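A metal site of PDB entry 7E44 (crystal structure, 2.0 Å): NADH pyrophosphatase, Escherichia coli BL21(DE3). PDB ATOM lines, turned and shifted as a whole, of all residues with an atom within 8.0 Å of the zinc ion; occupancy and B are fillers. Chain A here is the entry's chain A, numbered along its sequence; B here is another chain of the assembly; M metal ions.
A ring nitrogen (ND1) of His 105 lies close to the side-chain sulfur (SG) of Cys 103 (3.4 Å).
SG of Cys 100 lies close to N of Tyr 102 (3.5 Å).
The backbone carbonyl oxygen (O) of His 105 lies within hydrogen-bond range of the backbone NH (N) of Cys 100 (2.7 Å).
The backbone carbonyl oxygen (O) of Glu 123 sits at hydrogen-bond distance from the backbone NH (N) of Cys 118 (3.3 Å).
SG of Cys 118 sits close to N of His 120.
The nearest printed residue that does not touch the zinc ion is Tyr 102 (4.6 Å).
The zinc ion is bound by the side-chain sulfur (SG) of Cys 121 (2.2 Å).
The zinc ion is bound by the side-chain sulfur (SG) of Cys 118 (2.3 Å).
The zinc ion is bound by the side-chain sulfur (SG) of Cys 103 (2.3 Å).
The side-chain sulfur (SG) of Cys 100 is bound to the zinc ion.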
ATOM      1  N   TYR A  99      -8.188  24.644   0.353  1.00  0.00           N
ATOM      2  CA  TYR A  99      -7.690  23.974   1.582  1.00  0.00           C
ATOM      3  C   TYR A  99      -7.278  22.551   1.196  1.00  0.00           C
ATOM      4  O   TYR A  99      -7.942  21.962   0.362  1.00  0.00           O
ATOM      5  CB  TYR A  99      -8.793  23.975   2.646  1.00  0.00           C
ATOM      6  CG  TYR A  99      -9.272  25.353   3.018  1.00  0.00           C
ATOM      7  CD1 TYR A  99     -10.315  25.957   2.349  1.00  0.00           C
ATOM      8  CD2 TYR A  99      -8.683  26.048   4.066  1.00  0.00           C
ATOM      9  CE1 TYR A  99     -10.761  27.223   2.687  1.00  0.00           C
ATOM     10  CE2 TYR A  99      -9.115  27.317   4.421  1.00  0.00           C
ATOM     11  CZ  TYR A  99     -10.163  27.903   3.737  1.00  0.00           C
ATOM     12  OH  TYR A  99     -10.584  29.145   4.088  1.00  0.00           O
ATOM     13  N   CYS A 100      -6.186  22.053   1.765  1.00  0.00           N
ATOM     14  CA  CYS A 100      -5.712  20.696   1.427  1.00  0.00           C
ATOM     15  C   CYS A 100      -6.665  19.656   2.030  1.00  0.00           C
ATOM     16  O   CYS A 100      -6.973  19.764   3.213  1.00  0.00           O
ATOM     17  CB  CYS A 100      -4.284  20.524   1.915  1.00  0.00           C
ATOM     18  SG  CYS A 100      -3.735  18.817   2.076  1.00  0.00           S
ATOM     19  N   GLY A 101      -7.086  18.675   1.232  1.00  0.00           N
ATOM     20  CA  GLY A 101      -8.028  17.642   1.685  1.00  0.00           C
ATOM     21  C   GLY A 101      -7.463  16.773   2.794  1.00  0.00           C
ATOM     22  O   GLY A 101      -8.240  16.392   3.681  1.00  0.00           O
ATOM     23  N   TYR A 102      -6.179  16.425   2.699  1.00  0.00           N
ATOM     24  CA  TYR A 102      -5.525  15.566   3.711  1.00  0.00           C
ATOM     25  C   TYR A 102      -5.388  16.248   5.077  1.00  0.00           C
ATOM     26  O   TYR A 102      -5.685  15.580   6.068  1.00  0.00           O
ATOM     27  CB  TYR A 102      -4.128  15.159   3.265  1.00  0.00           C
ATOM     28  CG  TYR A 102      -4.019  14.390   1.966  1.00  0.00           C
ATOM     29  CD1 TYR A 102      -3.974  15.049   0.756  1.00  0.00           C
ATOM     30  CD2 TYR A 102      -3.938  13.014   1.959  1.00  0.00           C
ATOM     31  CE1 TYR A 102      -3.871  14.363  -0.437  1.00  0.00           C
ATOM     32  CE2 TYR A 102      -3.825  12.301   0.776  1.00  0.00           C
ATOM     33  CZ  TYR A 102      -3.792  12.975  -0.422  1.00  0.00           C
ATOM     34  OH  TYR A 102      -3.683  12.296  -1.593  1.00  0.00           O
ATOM     35  N   CYS A 103      -4.964  17.517   5.140  1.00  0.00           N
ATOM     36  CA  CYS A 103      -4.683  18.134   6.472  1.00  0.00           C
ATOM     37  C   CYS A 103      -5.503  19.398   6.798  1.00  0.00           C
ATOM     38  O   CYS A 103      -5.438  19.821   7.958  1.00  0.00           O
ATOM     39  CB  CYS A 103      -3.192  18.423   6.624  1.00  0.00           C
ATOM     40  SG  CYS A 103      -2.627  19.868   5.688  1.00  0.00           S
ATOM     41  N   GLY A 104      -6.212  19.981   5.830  1.00  0.00           N
ATOM     42  CA  GLY A 104      -7.033  21.184   6.099  1.00  0.00           C
ATOM     43  C   GLY A 104      -6.265  22.486   5.937  1.00  0.00           C
ATOM     44  O   GLY A 104      -6.910  23.536   5.977  1.00  0.00           O
ATOM     45  N   HIS A 105      -4.945  22.416   5.749  1.00  0.00           N
ATOM     46  CA  HIS A 105      -4.105  23.649   5.618  1.00  0.00           C
ATOM     47  C   HIS A 105      -4.312  24.316   4.255  1.00  0.00           C
ATOM     48  O   HIS A 105      -4.652  23.609   3.288  1.00  0.00           O
ATOM     49  CB  HIS A 105      -2.640  23.350   5.942  1.00  0.00           C
ATOM     50  CG  HIS A 105      -2.370  23.343   7.414  1.00  0.00           C
ATOM     51  ND1 HIS A 105      -2.378  22.184   8.150  1.00  0.00           N
ATOM     52  CD2 HIS A 105      -2.108  24.338   8.272  1.00  0.00           C
ATOM     53  CE1 HIS A 105      -2.122  22.465   9.404  1.00  0.00           C
ATOM     54  NE2 HIS A 105      -1.960  23.775   9.513  1.00  0.00           N
ATOM     55  N   GLU A 106      -4.094  25.625   4.173  1.00  0.00           N
ATOM     56  CA  GLU A 106      -4.243  26.368   2.900  1.00  0.00           C
ATOM     57  C   GLU A 106      -3.199  25.859   1.899  1.00  0.00           C
ATOM     58  O   GLU A 106      -2.066  25.575   2.313  1.00  0.00           O
ATOM     59  CB  GLU A 106      -4.213  27.874   3.130  1.00  0.00           C
ATOM     60  CG  GLU A 106      -5.557  28.446   3.555  1.00  0.00           C
ATOM     61  CD  GLU A 106      -5.584  29.908   3.983  1.00  0.00           C
ATOM     62  OE1 GLU A 106      -4.615  30.630   3.672  1.00  0.00           O
ATOM     63  OE2 GLU A 106      -6.575  30.310   4.615  1.00  0.00           O
ATOM     64  N   MET A 107      -3.579  25.747   0.630  1.00  0.00           N
ATOM     65  CA  MET A 107      -2.693  25.229  -0.440  1.00  0.00           C
ATOM     66  C   MET A 107      -2.236  26.389  -1.328  1.00  0.00           C
ATOM     67  O   MET A 107      -2.855  27.449  -1.275  1.00  0.00           O
ATOM     68  CB  MET A 107      -3.428  24.212  -1.309  1.00  0.00           C
ATOM     69  CG  MET A 107      -3.906  22.994  -0.561  1.00  0.00           C
ATOM     70  SD  MET A 107      -4.281  21.642  -1.696  1.00  0.00           S
ATOM     71  CE  MET A 107      -2.810  20.655  -1.531  1.00  0.00           C
ATOM     72  N   LEU A 117      -0.204  22.661  -4.280  1.00  0.00           N
ATOM     73  CA  LEU A 117       0.763  22.069  -3.309  1.00  0.00           C
ATOM     74  C   LEU A 117       0.363  22.489  -1.891  1.00  0.00           C
ATOM     75  O   LEU A 117      -0.110  23.613  -1.707  1.00  0.00           O
ATOM     76  CB  LEU A 117       2.174  22.544  -3.661  1.00  0.00           C
ATOM     77  CG  LEU A 117       2.543  22.464  -5.136  1.00  0.00           C
ATOM     78  CD1 LEU A 117       4.028  22.737  -5.325  1.00  0.00           C
ATOM     79  CD2 LEU A 117       2.187  21.116  -5.726  1.00  0.00           C
ATOM     80  N   CYS A 118       0.591  21.610  -0.916  1.00  0.00           N
ATOM     81  CA  CYS A 118       0.195  21.942   0.469  1.00  0.00           C
ATOM     82  C   CYS A 118       1.371  22.527   1.257  1.00  0.00           C
ATOM     83  O   CYS A 118       2.477  21.972   1.194  1.00  0.00           O
ATOM     84  CB  CYS A 118      -0.342  20.731   1.204  1.00  0.00           C
ATOM     85  SG  CYS A 118      -0.972  21.141   2.850  1.00  0.00           S
ATOM     86  N   SER A 119       1.099  23.630   1.945  1.00  0.00           N
ATOM     87  CA  SER A 119       2.052  24.368   2.807  1.00  0.00           C
ATOM     88  C   SER A 119       2.500  23.505   3.986  1.00  0.00           C
ATOM     89  O   SER A 119       3.640  23.668   4.443  1.00  0.00           O
ATOM     90  CB  SER A 119       1.431  25.650   3.289  1.00  0.00           C
ATOM     91  OG  SER A 119       0.304  25.371   4.101  1.00  0.00           O
ATOM     92  N   HIS A 120       1.588  22.705   4.527  1.00  0.00           N
ATOM     93  CA  HIS A 120       1.857  21.878   5.726  1.00  0.00           C
ATOM     94  C   HIS A 120       2.238  20.434   5.364  1.00  0.00           C
ATOM     95  O   HIS A 120       3.207  19.916   5.936  1.00  0.00           O
ATOM     96  CB  HIS A 120       0.625  21.952   6.625  1.00  0.00           C
ATOM     97  CG  HIS A 120       0.710  21.215   7.914  1.00  0.00           C
ATOM     98  ND1 HIS A 120       1.280  21.770   9.032  1.00  0.00           N
ATOM     99  CD2 HIS A 120       0.247  20.009   8.282  1.00  0.00           C
ATOM    100  CE1 HIS A 120       1.191  20.926  10.034  1.00  0.00           C
ATOM    101  NE2 HIS A 120       0.567  19.836   9.594  1.00  0.00           N
ATOM    102  N   CYS A 121       1.489  19.814   4.448  1.00  0.00           N
ATOM    103  CA  CYS A 121       1.683  18.409   4.002  1.00  0.00           C
ATOM    104  C   CYS A 121       2.712  18.245   2.912  1.00  0.00           C
ATOM    105  O   CYS A 121       3.124  19.228   2.314  1.00  0.00           O
ATOM    106  CB  CYS A 121       0.597  18.019   3.012  1.00  0.00           C
ATOM    107  SG  CYS A 121      -0.835  17.206   3.706  1.00  0.00           S
ATOM    108  N   ARG A 122       2.980  16.984   2.594  1.00  0.00           N
ATOM    109  CA  ARG A 122       3.818  16.627   1.439  1.00  0.00           C
ATOM    110  C   ARG A 122       2.890  16.401   0.233  1.00  0.00           C
ATOM    111  O   ARG A 122       3.421  16.384  -0.892  1.00  0.00           O
ATOM    112  CB  ARG A 122       4.595  15.344   1.748  1.00  0.00           C
ATOM    113  CG  ARG A 122       5.972  15.284   1.096  1.00  0.00           C
ATOM    114  CD  ARG A 122       6.676  13.962   1.361  1.00  0.00           C
ATOM    115  NE  ARG A 122       7.945  14.137   2.026  1.00  0.00           N
ATOM    116  CZ  ARG A 122       9.026  13.419   1.787  1.00  0.00           C
ATOM    117  NH1 ARG A 122       8.989  12.455   0.881  1.00  0.00           N
ATOM    118  NH2 ARG A 122      10.151  13.661   2.449  1.00  0.00           N
ATOM    119  N   GLU A 123       1.564  16.317   0.443  1.00  0.00           N
ATOM    120  CA  GLU A 123       0.605  15.985  -0.638  1.00  0.00           C
ATOM    121  C   GLU A 123       0.311  17.117  -1.631  1.00  0.00           C
ATOM    122  O   GLU A 123       0.487  18.292  -1.299  1.00  0.00           O
ATOM    123  CB  GLU A 123      -0.695  15.481  -0.009  1.00  0.00           C
ATOM    124  CG  GLU A 123      -0.480  14.518   1.137  1.00  0.00           C
ATOM    125  CD  GLU A 123       0.050  13.151   0.740  1.00  0.00           C
ATOM    126  OE1 GLU A 123       0.106  12.863  -0.457  1.00  0.00           O
ATOM    127  OE2 GLU A 123       0.411  12.382   1.638  1.00  0.00           O
ATOM    128  N   ARG A 124      -0.094  16.725  -2.848  1.00  0.00           N
ATOM    129  CA  ARG A 124      -0.448  17.650  -3.951  1.00  0.00           C
ATOM    130  C   ARG A 124      -1.665  17.114  -4.699  1.00  0.00           C
ATOM    131  O   ARG A 124      -1.991  15.928  -4.548  1.00  0.00           O
ATOM    132  CB  ARG A 124       0.721  17.778  -4.925  1.00  0.00           C
ATOM    133  CG  ARG A 124       1.088  16.464  -5.596  1.00  0.00           C
ATOM    134  CD  ARG A 124       2.360  16.564  -6.410  1.00  0.00           C
ATOM    135  NE  ARG A 124       3.427  17.170  -5.659  1.00  0.00           N
ATOM    136  CZ  ARG A 124       4.488  17.746  -6.208  1.00  0.00           C
ATOM    137  NH1 ARG A 124       4.602  17.794  -7.515  1.00  0.00           N
ATOM    138  NH2 ARG A 124       5.424  18.290  -5.440  1.00  0.00           N
ATOM    139  N   TYR A 125      -2.330  17.981  -5.460  1.00  0.00           N
ATOM    140  CA  TYR A 125      -3.499  17.561  -6.280  1.00  0.00           C
ATOM    141  C   TYR A 125      -3.316  18.073  -7.718  1.00  0.00           C
ATOM    142  O   TYR A 125      -2.755  19.153  -7.897  1.00  0.00           O
ATOM    143  CB  TYR A 125      -4.778  18.207  -5.770  1.00  0.00           C
ATOM    144  CG  TYR A 125      -5.214  17.730  -4.414  1.00  0.00           C
ATOM    145  CD1 TYR A 125      -5.976  16.593  -4.283  1.00  0.00           C
ATOM    146  CD2 TYR A 125      -4.867  18.431  -3.272  1.00  0.00           C
ATOM    147  CE1 TYR A 125      -6.402  16.154  -3.041  1.00  0.00           C
ATOM    148  CE2 TYR A 125      -5.279  18.007  -2.020  1.00  0.00           C
ATOM    149  CZ  TYR A 125      -6.047  16.863  -1.912  1.00  0.00           C
ATOM    150  OH  TYR A 125      -6.463  16.432  -0.697  1.00  0.00           O
ATOM    151  N   TYR B  99     -10.830  16.741   4.632  1.00  0.00           N
ATOM    152  CA  TYR B  99     -11.234  18.164   4.687  1.00  0.00           C
ATOM    153  C   TYR B  99     -11.711  18.593   3.301  1.00  0.00           C
ATOM    154  O   TYR B  99     -11.159  18.126   2.298  1.00  0.00           O
ATOM    155  CB  TYR B  99     -10.092  19.040   5.210  1.00  0.00           C
ATOM    156  CG  TYR B  99      -9.643  18.711   6.610  1.00  0.00           C
ATOM    157  CD1 TYR B  99     -10.289  19.238   7.700  1.00  0.00           C
ATOM    158  CD2 TYR B  99      -8.596  17.842   6.822  1.00  0.00           C
ATOM    159  CE1 TYR B  99      -9.897  18.922   8.994  1.00  0.00           C
ATOM    160  CE2 TYR B  99      -8.181  17.505   8.106  1.00  0.00           C
ATOM    161  CZ  TYR B  99      -8.841  18.050   9.187  1.00  0.00           C
ATOM    162  OH  TYR B  99      -8.440  17.742  10.453  1.00  0.00           O
HETATM  163 ZN    ZN M   1      -1.898  19.181   3.599  1.00  0.00          ZN
